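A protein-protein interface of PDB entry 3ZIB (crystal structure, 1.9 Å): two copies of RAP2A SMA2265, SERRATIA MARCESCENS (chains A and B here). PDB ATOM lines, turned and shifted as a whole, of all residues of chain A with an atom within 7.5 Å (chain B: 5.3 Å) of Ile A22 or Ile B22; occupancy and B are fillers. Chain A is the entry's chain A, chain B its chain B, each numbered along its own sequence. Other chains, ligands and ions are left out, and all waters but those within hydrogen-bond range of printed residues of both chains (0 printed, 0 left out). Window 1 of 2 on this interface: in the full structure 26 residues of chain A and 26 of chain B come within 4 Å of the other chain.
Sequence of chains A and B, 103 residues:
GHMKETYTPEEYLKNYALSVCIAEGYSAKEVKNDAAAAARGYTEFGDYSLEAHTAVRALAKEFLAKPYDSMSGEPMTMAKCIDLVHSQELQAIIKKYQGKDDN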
ATOM      1  N   TYR A  16       2.099 -17.998   1.261  1.00  0.00           N
ATOM      2  CA  TYR A  16       0.783 -18.624   1.403  1.00  0.00           C
ATOM      3  C   TYR A  16       0.566 -18.979   2.905  1.00  0.00           C
ATOM      4  O   TYR A  16      -0.491 -18.685   3.465  1.00  0.00           O
ATOM      5  CB  TYR A  16       0.740 -19.918   0.563  1.00  0.00           C
ATOM      6  CG  TYR A  16      -0.498 -20.747   0.884  1.00  0.00           C
ATOM      7  CD1 TYR A  16      -1.765 -20.371   0.405  1.00  0.00           C
ATOM      8  CD2 TYR A  16      -0.404 -21.877   1.683  1.00  0.00           C
ATOM      9  CE1 TYR A  16      -2.917 -21.095   0.727  1.00  0.00           C
ATOM     10  CE2 TYR A  16      -1.536 -22.610   2.010  1.00  0.00           C
ATOM     11  CZ  TYR A  16      -2.769 -22.237   1.512  1.00  0.00           C
ATOM     12  OH  TYR A  16      -3.843 -22.990   1.855  1.00  0.00           O
ATOM     13  N   ALA A  17       1.570 -19.606   3.541  1.00  0.00           N
ATOM     14  CA  ALA A  17       1.462 -19.935   4.941  1.00  0.00           C
ATOM     15  C   ALA A  17       1.069 -18.711   5.762  1.00  0.00           C
ATOM     16  O   ALA A  17       0.167 -18.761   6.634  1.00  0.00           O
ATOM     17  CB  ALA A  17       2.776 -20.532   5.462  1.00  0.00           C
ATOM     18  N   LEU A  18       1.793 -17.600   5.551  1.00  0.00           N
ATOM     19  CA  LEU A  18       1.464 -16.435   6.392  1.00  0.00           C
ATOM     20  C   LEU A  18       0.036 -15.973   6.137  1.00  0.00           C
ATOM     21  O   LEU A  18      -0.693 -15.609   7.082  1.00  0.00           O
ATOM     22  CB  LEU A  18       2.439 -15.266   6.079  1.00  0.00           C
ATOM     23  CG  LEU A  18       2.237 -13.966   6.854  1.00  0.00           C
ATOM     24  CD1 LEU A  18       2.393 -14.165   8.339  1.00  0.00           C
ATOM     25  CD2 LEU A  18       3.358 -13.075   6.311  1.00  0.00           C
ATOM     26  N   SER A  19      -0.302 -15.833   4.869  1.00  0.00           N
ATOM     27  CA  SER A  19      -1.628 -15.338   4.445  1.00  0.00           C
ATOM     28  C   SER A  19      -2.783 -16.181   4.955  1.00  0.00           C
ATOM     29  O   SER A  19      -3.746 -15.661   5.513  1.00  0.00           O
ATOM     30  CB  SER A  19      -1.694 -15.276   2.897  1.00  0.00           C
ATOM     31  OG  SER A  19      -0.678 -14.415   2.451  1.00  0.00           O
ATOM     32  N   VAL A  20      -2.701 -17.483   4.815  1.00  0.00           N
ATOM     33  CA  VAL A  20      -3.761 -18.350   5.371  1.00  0.00           C
ATOM     34  C   VAL A  20      -3.815 -18.343   6.895  1.00  0.00           C
ATOM     35  O   VAL A  20      -4.923 -18.440   7.505  1.00  0.00           O
ATOM     36  CB  VAL A  20      -3.713 -19.866   4.893  1.00  0.00           C
ATOM     37  CG1 VAL A  20      -3.954 -19.955   3.400  1.00  0.00           C
ATOM     38  CG2 VAL A  20      -2.420 -20.553   5.299  1.00  0.00           C
ATOM     39  N   CYS A  21      -2.636 -18.268   7.521  1.00  0.00           N
ATOM     40  CA  CYS A  21      -2.594 -18.170   8.973  1.00  0.00           C
ATOM     41  C   CYS A  21      -3.345 -16.916   9.472  1.00  0.00           C
ATOM     42  O   CYS A  21      -4.239 -17.007  10.373  1.00  0.00           O
ATOM     43  CB  CYS A  21      -1.149 -18.212   9.460  1.00  0.00           C
ATOM     44  SG  CYS A  21      -0.995 -18.296  11.270  1.00  0.00           S
ATOM     45  N   ILE A  22      -3.044 -15.768   8.885  1.00  0.00           N
ATOM     46  CA  ILE A  22      -3.751 -14.554   9.259  1.00  0.00           C
ATOM     47  C   ILE A  22      -5.262 -14.586   8.933  1.00  0.00           C
ATOM     48  O   ILE A  22      -6.105 -14.130   9.776  1.00  0.00           O
ATOM     49  CB  ILE A  22      -2.981 -13.312   8.719  1.00  0.00           C
ATOM     50  CG1 ILE A  22      -1.625 -13.271   9.429  1.00  0.00           C
ATOM     51  CG2 ILE A  22      -3.753 -12.021   8.958  1.00  0.00           C
ATOM     52  CD1 ILE A  22      -0.602 -12.380   8.770  1.00  0.00           C
ATOM     53  N   ALA A  23      -5.622 -15.162   7.774  1.00  0.00           N
ATOM     54  CA  ALA A  23      -7.049 -15.342   7.371  1.00  0.00           C
ATOM     55  C   ALA A  23      -7.823 -16.268   8.348  1.00  0.00           C
ATOM     56  O   ALA A  23      -8.965 -15.946   8.736  1.00  0.00           O
ATOM     57  CB  ALA A  23      -7.160 -15.896   5.922  1.00  0.00           C
ATOM     58  N   GLU A  24      -7.178 -17.356   8.790  1.00  0.00           N
ATOM     59  CA  GLU A  24      -7.727 -18.262   9.820  1.00  0.00           C
ATOM     60  C   GLU A  24      -7.728 -17.661  11.230  1.00  0.00           C
ATOM     61  O   GLU A  24      -8.617 -17.957  12.016  1.00  0.00           O
ATOM     62  CB  GLU A  24      -7.003 -19.621   9.849  1.00  0.00           C
ATOM     63  CG  GLU A  24      -7.141 -20.382   8.563  1.00  0.00           C
ATOM     64  CD  GLU A  24      -8.562 -20.970   8.361  1.00  0.00           C
ATOM     65  OE1 GLU A  24      -9.305 -21.178   9.362  1.00  0.00           O
ATOM     66  OE2 GLU A  24      -8.931 -21.211   7.175  1.00  0.00           O
ATOM     67  N   GLY A  25      -6.775 -16.802  11.551  1.00  0.00           N
ATOM     68  CA  GLY A  25      -6.576 -16.493  12.933  1.00  0.00           C
ATOM     69  C   GLY A  25      -7.358 -15.274  13.364  1.00  0.00           C
ATOM     70  O   GLY A  25      -7.460 -15.046  14.551  1.00  0.00           O
ATOM     71  N   TYR A  26      -7.912 -14.493  12.444  1.00  0.00           N
ATOM     72  CA  TYR A  26      -8.688 -13.333  12.876  1.00  0.00           C
ATOM     73  C   TYR A  26     -10.117 -13.514  12.444  1.00  0.00           C
ATOM     74  O   TYR A  26     -10.348 -14.144  11.428  1.00  0.00           O
ATOM     75  CB  TYR A  26      -8.154 -12.051  12.233  1.00  0.00           C
ATOM     76  CG  TYR A  26      -6.820 -11.578  12.803  1.00  0.00           C
ATOM     77  CD1 TYR A  26      -6.675 -11.267  14.154  1.00  0.00           C
ATOM     78  CD2 TYR A  26      -5.698 -11.383  11.943  1.00  0.00           C
ATOM     79  CE1 TYR A  26      -5.485 -10.803  14.667  1.00  0.00           C
ATOM     80  CE2 TYR A  26      -4.477 -10.919  12.459  1.00  0.00           C
ATOM     81  CZ  TYR A  26      -4.382 -10.628  13.825  1.00  0.00           C
ATOM     82  OH  TYR A  26      -3.184 -10.206  14.327  1.00  0.00           O
ATOM     83  N   SER A  27     -11.066 -12.976  13.213  1.00  0.00           N
ATOM     84  CA  SER A  27     -12.494 -13.037  12.816  1.00  0.00           C
ATOM     85  C   SER A  27     -12.977 -11.918  11.893  1.00  0.00           C
ATOM     86  O   SER A  27     -13.867 -12.138  11.073  1.00  0.00           O
ATOM     87  CB  SER A  27     -13.455 -13.220  14.028  1.00  0.00           C
ATOM     88  OG  SER A  27     -12.934 -12.640  15.195  1.00  0.00           O
ATOM     89  N   ALA A  28     -12.377 -10.734  11.977  1.00  0.00           N
ATOM     90  CA  ALA A  28     -12.806  -9.606  11.144  1.00  0.00           C
ATOM     91  C   ALA A  28     -12.900 -10.000   9.672  1.00  0.00           C
ATOM     92  O   ALA A  28     -11.901 -10.368   9.057  1.00  0.00           O
ATOM     93  CB  ALA A  28     -11.862  -8.397  11.344  1.00  0.00           C
ATOM     94  N   GLU A  30     -13.126  -8.152   7.118  1.00  0.00           N
ATOM     95  CA  GLU A  30     -12.213  -7.285   6.351  1.00  0.00           C
ATOM     96  C   GLU A  30     -10.879  -8.029   6.114  1.00  0.00           C
ATOM     97  O   GLU A  30     -10.358  -8.080   5.015  1.00  0.00           O
ATOM     98  CB  GLU A  30     -11.929  -5.995   7.132  1.00  0.00           C
ATOM     99  CG  GLU A  30     -10.913  -5.076   6.486  1.00  0.00           C
ATOM    100  CD  GLU A  30     -10.230  -4.083   7.442  1.00  0.00           C
ATOM    101  OE1 GLU A  30     -10.470  -4.047   8.663  1.00  0.00           O
ATOM    102  OE2 GLU A  30      -9.392  -3.311   6.965  1.00  0.00           O
ATOM    103  N   VAL A  31     -10.346  -8.591   7.181  1.00  0.00           N
ATOM    104  CA  VAL A  31      -9.037  -9.206   7.111  1.00  0.00           C
ATOM    105  C   VAL A  31      -9.113 -10.619   6.560  1.00  0.00           C
ATOM    106  O   VAL A  31      -8.299 -10.957   5.690  1.00  0.00           O
ATOM    107  CB  VAL A  31      -8.343  -9.183   8.484  1.00  0.00           C
ATOM    108  CG1 VAL A  31      -6.981  -9.861   8.400  1.00  0.00           C
ATOM    109  CG2 VAL A  31      -8.219  -7.748   8.977  1.00  0.00           C
ATOM    110  N   LYS A  32     -10.081 -11.426   7.007  1.00  0.00           N
ATOM    111  CA  LYS A  32     -10.214 -12.778   6.438  1.00  0.00           C
ATOM    112  C   LYS A  32     -10.284 -12.732   4.922  1.00  0.00           C
ATOM    113  O   LYS A  32      -9.594 -13.499   4.260  1.00  0.00           O
ATOM    114  CB  LYS A  32     -11.399 -13.614   6.972  1.00  0.00           C
ATOM    115  CG  LYS A  32     -11.509 -13.701   8.473  1.00  0.00           C
ATOM    116  CD  LYS A  32     -12.658 -14.636   8.890  1.00  0.00           C
ATOM    117  CE  LYS A  32     -12.225 -16.057   8.843  1.00  0.00           C
ATOM    118  NZ  LYS A  32     -11.354 -16.420   9.995  1.00  0.00           N
ATOM    119  N   ALA A  35      -6.727 -11.292   3.325  1.00  0.00           N
ATOM    120  CA  ALA A  35      -5.618 -12.301   3.446  1.00  0.00           C
ATOM    121  C   ALA A  35      -5.943 -13.580   2.646  1.00  0.00           C
ATOM    122  O   ALA A  35      -5.051 -14.159   1.991  1.00  0.00           O
ATOM    123  CB  ALA A  35      -5.350 -12.629   4.948  1.00  0.00           C
ATOM    124  N   ALA A  36      -7.213 -14.042   2.695  1.00  0.00           N
ATOM    125  CA  ALA A  36      -7.666 -15.138   1.776  1.00  0.00           C
ATOM    126  C   ALA A  36      -7.389 -14.865   0.286  1.00  0.00           C
ATOM    127  O   ALA A  36      -6.990 -15.787  -0.449  1.00  0.00           O
ATOM    128  CB  ALA A  36      -9.122 -15.468   1.984  1.00  0.00           C
ATOM    129  N   ALA A  60      -0.718 -24.289   9.855  1.00  0.00           N
ATOM    130  CA  ALA A  60      -1.125 -22.967  10.337  1.00  0.00           C
ATOM    131  C   ALA A  60      -2.189 -23.074  11.443  1.00  0.00           C
ATOM    132  O   ALA A  60      -2.122 -22.426  12.512  1.00  0.00           O
ATOM    133  CB  ALA A  60      -1.651 -22.112   9.188  1.00  0.00           C
ATOM    134  N   LEU A  64      -1.974 -21.678  15.338  1.00  0.00           N
ATOM    135  CA  LEU A  64      -3.006 -20.802  15.889  1.00  0.00           C
ATOM    136  C   LEU A  64      -3.645 -21.430  17.122  1.00  0.00           C
ATOM    137  O   LEU A  64      -4.085 -20.725  18.041  1.00  0.00           O
ATOM    138  CB  LEU A  64      -4.070 -20.550  14.840  1.00  0.00           C
ATOM    139  CG  LEU A  64      -3.657 -19.625  13.684  1.00  0.00           C
ATOM    140  CD1 LEU A  64      -4.687 -19.728  12.549  1.00  0.00           C
ATOM    141  CD2 LEU A  64      -3.493 -18.207  14.181  1.00  0.00           C
ATOM    142  N   THR A  77      -2.161 -13.786  17.729  1.00  0.00           N
ATOM    143  CA  THR A  77      -2.207 -14.306  16.371  1.00  0.00           C
ATOM    144  C   THR A  77      -1.033 -13.862  15.483  1.00  0.00           C
ATOM    145  O   THR A  77      -0.474 -14.657  14.716  1.00  0.00           O
ATOM    146  CB  THR A  77      -3.504 -13.841  15.742  1.00  0.00           C
ATOM    147  OG1 THR A  77      -4.573 -14.411  16.499  1.00  0.00           O
ATOM    148  CG2 THR A  77      -3.624 -14.360  14.314  1.00  0.00           C
ATOM    149  N   MET A  78      -0.714 -12.561  15.508  1.00  0.00           N
ATOM    150  CA  MET A  78       0.305 -12.087  14.612  1.00  0.00           C
ATOM    151  C   MET A  78       1.589 -12.831  14.906  1.00  0.00           C
ATOM    152  O   MET A  78       2.248 -13.309  13.995  1.00  0.00           O
ATOM    153  CB  MET A  78       0.484 -10.537  14.738  1.00  0.00           C
ATOM    154  CG  MET A  78       1.539  -9.979  13.785  1.00  0.00           C
ATOM    155  SD  MET A  78       0.902  -9.904  12.081  1.00  0.00           S
ATOM    156  CE  MET A  78       1.776 -11.215  11.248  1.00  0.00           C
ATOM    157  N   CYS A  81       1.578 -16.572  13.686  1.00  0.00           N
ATOM    158  CA  CYS A  81       1.741 -16.713  12.220  1.00  0.00           C
ATOM    159  C   CYS A  81       3.215 -16.430  11.792  1.00  0.00           C
ATOM    160  O   CYS A  81       3.734 -17.042  10.877  1.00  0.00           O
ATOM    161  CB  CYS A  81       0.777 -15.784  11.512  1.00  0.00           C
ATOM    162  SG  CYS A  81      -0.964 -16.331  11.831  1.00  0.00           S
ATOM    163  N   ILE A  82       3.824 -15.440  12.435  1.00  0.00           N
ATOM    164  CA  ILE A  82       5.239 -15.164  12.189  1.00  0.00           C
ATOM    165  C   ILE A  82       6.109 -16.349  12.600  1.00  0.00           C
ATOM    166  O   ILE A  82       7.052 -16.755  11.865  1.00  0.00           O
ATOM    167  CB  ILE A  82       5.632 -13.893  12.940  1.00  0.00           C
ATOM    168  CG1 ILE A  82       5.169 -12.712  12.099  1.00  0.00           C
ATOM    169  CG2 ILE A  82       7.167 -13.832  13.066  1.00  0.00           C
ATOM    170  CD1 ILE A  82       5.342 -11.353  12.738  1.00  0.00           C
ATOM    171  N   LEU A  84       5.099 -19.487  12.758  1.00  0.00           N
ATOM    172  CA  LEU A  84       4.773 -20.537  11.749  1.00  0.00           C
ATOM    173  C   LEU A  84       5.732 -20.384  10.536  1.00  0.00           C
ATOM    174  O   LEU A  84       6.342 -21.348  10.081  1.00  0.00           O
ATOM    175  CB  LEU A  84       3.317 -20.365  11.273  1.00  0.00           C
ATOM    176  CG  LEU A  84       2.903 -21.122   9.956  1.00  0.00           C
ATOM    177  CD1 LEU A  84       2.909 -22.608  10.241  1.00  0.00           C
ATOM    178  CD2 LEU A  84       1.549 -20.683   9.444  1.00  0.00           C
ATOM    179  N   ALA B  17       8.435  -4.971  11.110  1.00  0.00           N
ATOM    180  CA  ALA B  17       7.938  -4.385   9.856  1.00  0.00           C
ATOM    181  C   ALA B  17       6.624  -4.979   9.439  1.00  0.00           C
ATOM    182  O   ALA B  17       5.692  -4.274   9.095  1.00  0.00           O
ATOM    183  CB  ALA B  17       8.985  -4.606   8.724  1.00  0.00           C
ATOM    184  N   LEU B  18       6.523  -6.307   9.468  1.00  0.00           N
ATOM    185  CA  LEU B  18       5.254  -6.959   9.072  1.00  0.00           C
ATOM    186  C   LEU B  18       4.132  -6.649  10.034  1.00  0.00           C
ATOM    187  O   LEU B  18       3.024  -6.396   9.642  1.00  0.00           O
ATOM    188  CB  LEU B  18       5.490  -8.476   9.065  1.00  0.00           C
ATOM    189  CG  LEU B  18       4.224  -9.311   8.786  1.00  0.00           C
ATOM    190  CD1 LEU B  18       3.669  -9.067   7.392  1.00  0.00           C
ATOM    191  CD2 LEU B  18       4.620 -10.765   8.902  1.00  0.00           C
ATOM    192  N   SER B  19       4.430  -6.724  11.334  1.00  0.00           N
ATOM    193  CA  SER B  19       3.401  -6.373  12.398  1.00  0.00           C
ATOM    194  C   SER B  19       2.880  -4.921  12.288  1.00  0.00           C
ATOM    195  O   SER B  19       1.668  -4.654  12.334  1.00  0.00           O
ATOM    196  CB  SER B  19       4.052  -6.567  13.772  1.00  0.00           C
ATOM    197  OG  SER B  19       4.423  -7.928  13.910  1.00  0.00           O
ATOM    198  N   VAL B  20       3.787  -3.963  12.143  1.00  0.00           N
ATOM    199  CA  VAL B  20       3.322  -2.594  12.034  1.00  0.00           C
ATOM    200  C   VAL B  20       2.567  -2.402  10.731  1.00  0.00           C
ATOM    201  O   VAL B  20       1.617  -1.619  10.688  1.00  0.00           O
ATOM    202  CB  VAL B  20       4.453  -1.489  12.120  1.00  0.00           C
ATOM    203  CG1 VAL B  20       5.213  -1.546  13.457  1.00  0.00           C
ATOM    204  CG2 VAL B  20       5.425  -1.658  10.986  1.00  0.00           C
ATOM    205  N   CYS B  21       2.993  -3.090   9.656  1.00  0.00           N
ATOM    206  CA  CYS B  21       2.271  -2.955   8.388  1.00  0.00           C
ATOM    207  C   CYS B  21       0.834  -3.486   8.467  1.00  0.00           C
ATOM    208  O   CYS B  21      -0.110  -2.880   7.986  1.00  0.00           O
ATOM    209  CB  CYS B  21       3.087  -3.696   7.299  1.00  0.00           C
ATOM    210  SG  CYS B  21       2.433  -3.432   5.619  1.00  0.00           S
ATOM    211  N   ILE B  22       0.676  -4.682   9.033  1.00  0.00           N
ATOM    212  CA  ILE B  22      -0.654  -5.229   9.291  1.00  0.00           C
ATOM    213  C   ILE B  22      -1.471  -4.349  10.262  1.00  0.00           C
ATOM    214  O   ILE B  22      -2.674  -4.118  10.038  1.00  0.00           O
ATOM    215  CB  ILE B  22      -0.564  -6.712   9.736  1.00  0.00           C
ATOM    216  CG1 ILE B  22      -0.363  -7.561   8.489  1.00  0.00           C
ATOM    217  CG2 ILE B  22      -1.800  -7.168  10.513  1.00  0.00           C
ATOM    218  CD1 ILE B  22       0.181  -8.921   8.818  1.00  0.00           C
ATOM    219  N   ALA B  23      -0.836  -3.837  11.313  1.00  0.00           N
ATOM    220  CA  ALA B  23      -1.608  -2.914  12.241  1.00  0.00           C
ATOM    221  C   ALA B  23      -2.089  -1.622  11.565  1.00  0.00           C
ATOM    222  O   ALA B  23      -3.256  -1.193  11.759  1.00  0.00           O
ATOM    223  CB  ALA B  23      -0.782  -2.588  13.494  1.00  0.00           C
ATOM    224  N   GLU B  24      -1.218  -1.027  10.745  1.00  0.00           N
ATOM    225  CA  GLU B  24      -1.528   0.163   9.988  1.00  0.00           C
ATOM    226  C   GLU B  24      -2.458  -0.089   8.825  1.00  0.00           C
ATOM    227  O   GLU B  24      -3.215   0.795   8.433  1.00  0.00           O
ATOM    228  CB  GLU B  24      -0.269   0.784   9.375  1.00  0.00           C
ATOM    229  CG  GLU B  24       0.766   1.328  10.360  1.00  0.00           C
ATOM    230  CD  GLU B  24       0.292   2.630  11.017  1.00  0.00           C
ATOM    231  OE1 GLU B  24      -0.630   3.304  10.475  1.00  0.00           O
ATOM    232  OE2 GLU B  24       0.824   2.979  12.085  1.00  0.00           O
ATOM    233  N   GLY B  25      -2.352  -1.250   8.219  1.00  0.00           N
ATOM    234  CA  GLY B  25      -3.045  -1.514   6.995  1.00  0.00           C
ATOM    235  C   GLY B  25      -4.481  -1.883   7.096  1.00  0.00           C
ATOM    236  O   GLY B  25      -5.193  -1.737   6.137  1.00  0.00           O
ATOM    237  N   TYR B  26      -4.925  -2.422   8.226  1.00  0.00           N
ATOM    238  CA  TYR B  26      -6.322  -2.830   8.343  1.00  0.00           C
ATOM    239  C   TYR B  26      -7.117  -1.912   9.284  1.00  0.00           C
ATOM    240  O   TYR B  26      -6.537  -1.339  10.207  1.00  0.00           O
ATOM    241  CB  TYR B  26      -6.364  -4.269   8.896  1.00  0.00           C
ATOM    242  CG  TYR B  26      -5.927  -5.336   7.896  1.00  0.00           C
ATOM    243  CD1 TYR B  26      -6.600  -5.499   6.685  1.00  0.00           C
ATOM    244  CD2 TYR B  26      -4.835  -6.195   8.178  1.00  0.00           C
ATOM    245  CE1 TYR B  26      -6.225  -6.481   5.762  1.00  0.00           C
ATOM    246  CE2 TYR B  26      -4.454  -7.200   7.271  1.00  0.00           C
ATOM    247  CZ  TYR B  26      -5.151  -7.328   6.069  1.00  0.00           C
ATOM    248  OH  TYR B  26      -4.789  -8.329   5.158  1.00  0.00           O
ATOM    249  N   VAL B  31      -7.617  -6.574  14.791  1.00  0.00           N
ATOM    250  CA  VAL B  31      -6.335  -6.878  14.123  1.00  0.00           C
ATOM    251  C   VAL B  31      -5.380  -5.767  14.443  1.00  0.00           C
ATOM    252  O   VAL B  31      -4.221  -5.997  14.730  1.00  0.00           O
ATOM    253  CB  VAL B  31      -6.521  -7.054  12.590  1.00  0.00           C
ATOM    254  CG1 VAL B  31      -5.186  -7.408  11.926  1.00  0.00           C
ATOM    255  CG2 VAL B  31      -7.533  -8.154  12.320  1.00  0.00           C
ATOM    256  N   ALA B  35      -1.885  -6.870  16.191  1.00  0.00           N
ATOM    257  CA  ALA B  35      -0.664  -6.621  15.409  1.00  0.00           C
ATOM    258  C   ALA B  35       0.222  -5.537  16.039  1.00  0.00           C
ATOM    259  O   ALA B  35       1.438  -5.687  16.058  1.00  0.00           O
ATOM    260  CB  ALA B  35      -0.999  -6.303  13.906  1.00  0.00           C
ATOM    261  N   MET B  78      -2.498  -7.553   2.634  1.00  0.00           N
ATOM    262  CA  MET B  78      -1.646  -8.667   3.048  1.00  0.00           C
ATOM    263  C   MET B  78      -0.489  -8.762   2.042  1.00  0.00           C
ATOM    264  O   MET B  78       0.662  -8.914   2.469  1.00  0.00           O
ATOM    265  CB  MET B  78      -2.470  -9.981   3.111  1.00  0.00           C
ATOM    266  CG  MET B  78      -1.655 -11.193   3.568  1.00  0.00           C
ATOM    267  SD  MET B  78      -1.314 -11.139   5.360  1.00  0.00           S
ATOM    268  CE  MET B  78       0.388 -10.826   5.351  1.00  0.00           C
ATOM    269  N   CYS B  81       2.123  -5.945   2.564  1.00  0.00           N
ATOM    270  CA  CYS B  81       2.984  -6.130   3.706  1.00  0.00           C
ATOM    271  C   CYS B  81       4.000  -7.237   3.474  1.00  0.00           C
ATOM    272  O   CYS B  81       5.114  -7.193   4.024  1.00  0.00           O
ATOM    273  CB  CYS B  81       2.105  -6.418   4.952  1.00  0.00           C
ATOM    274  SG  CYS B  81       1.078  -4.989   5.394  1.00  0.00           S
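Of the 14 printed residues of chain B, 6 touch a printed residue of chain A.
Printed residues of chain B that touch a printed residue of chain A: Leu B18, Ser B19, Ile B22, Tyr B26, Val B31 and Met B78.
Hydrophobic or aromatic side chains of chain B that line the printed part of chain A: Leu B18, Ile B22, Tyr B26, Val B31 and Met B78.
Among the printed residues, 16 pairs touch across the chains.
Leu A18 touches Met B78, and with the chains exchanged Met A78 touches Leu B18.
Ile A22 touches its own counterpart, Ile B22.
Ala A35 touches Tyr B26, but with the chains exchanged Tyr A26 does not touch Ala B35 (4.04 Å).
Ala A35 touches Met B78, but with the chains exchanged Met A78 does not touch Ala B35 (4.1 Å).
Of the 16 pairs that touch across the chains among the printed residues, 11 have their exchanged pair printed and touching as well.
Leu B18 touches Leu A18 (CD2 to CD2, 3.7 Å).
CD2 of Leu A18 touches CE of Met B78 (3.8 Å).
Ile B22 touches Ile A22 (CD1 to CD1, 3.5 Å).
Glu A30 touches Tyr B26.
Tyr B26 touches Val A31 (CG to CG2, 3.5 Å).
CB of Met B78 touches CA of Ala A35, 3.9 Å away.
CE of Met A78 touches CD2 of Leu B18 (3.7 Å).
Ile B22 touches Met A78.
Leu B18 touches Ile A82.
CD1 of Ile A82 touches OG of Ser B19 (3.7 Å).
The backbone NH of Ile A22 is in hydrogen-bond range of the side-chain sulfur of Cys A81 (3.6 Å).
The side-chain amino group of Lys A32 sits at hydrogen-bond distance from the backbone carbonyl oxygen of Tyr A26.
N of Ile B22 lies within hydrogen-bond range of SG of Cys B81, 3.7 Å away.
The backbone NH of Met B78 sits at hydrogen-bond distance from the side-chain hydroxyl of Tyr B26 (3.5 Å).
The side-chain sulfur of Cys A21 is disulfide-bonded to the side-chain sulfur of Cys A81 (2.0 Å).
The side-chain sulfur of Cys B81 forms a disulfide with the side-chain sulfur of Cys B21 (2.1 Å).
Of the printed residues of chain B, Ser A19 touches Met B78.
Of the printed residues of chain B, Ile A22 touches Ile B22 (3.5 Å) and Met B78 (3.7 Å).
Of the printed residues of chain B, Tyr A26 touches Val B31.
Printed residues of chain B within 4 Å of Ile A82: Leu B18 and Ser B19.
Of the printed residues of chain A, Ile B22 touches Ile A22 (3.5 Å) and Met A78 (3.5 Å).
Of the printed residues of chain A, Tyr B26 touches Glu A30 (3.4 Å), Val A31 (3.5 Å) and Ala A35 (3.99 Å).
Printed residues of chain A within 4 Å of Met B78: Leu A18, Ser A19, Ile A22 and Ala A35.
The nearest printed residue of chain B that does not touch Ile A22 is Tyr B26 (5.2 Å).
The nearest printed residue of chain A that does not touch Ile B22 is Tyr A26 (5.0 Å).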
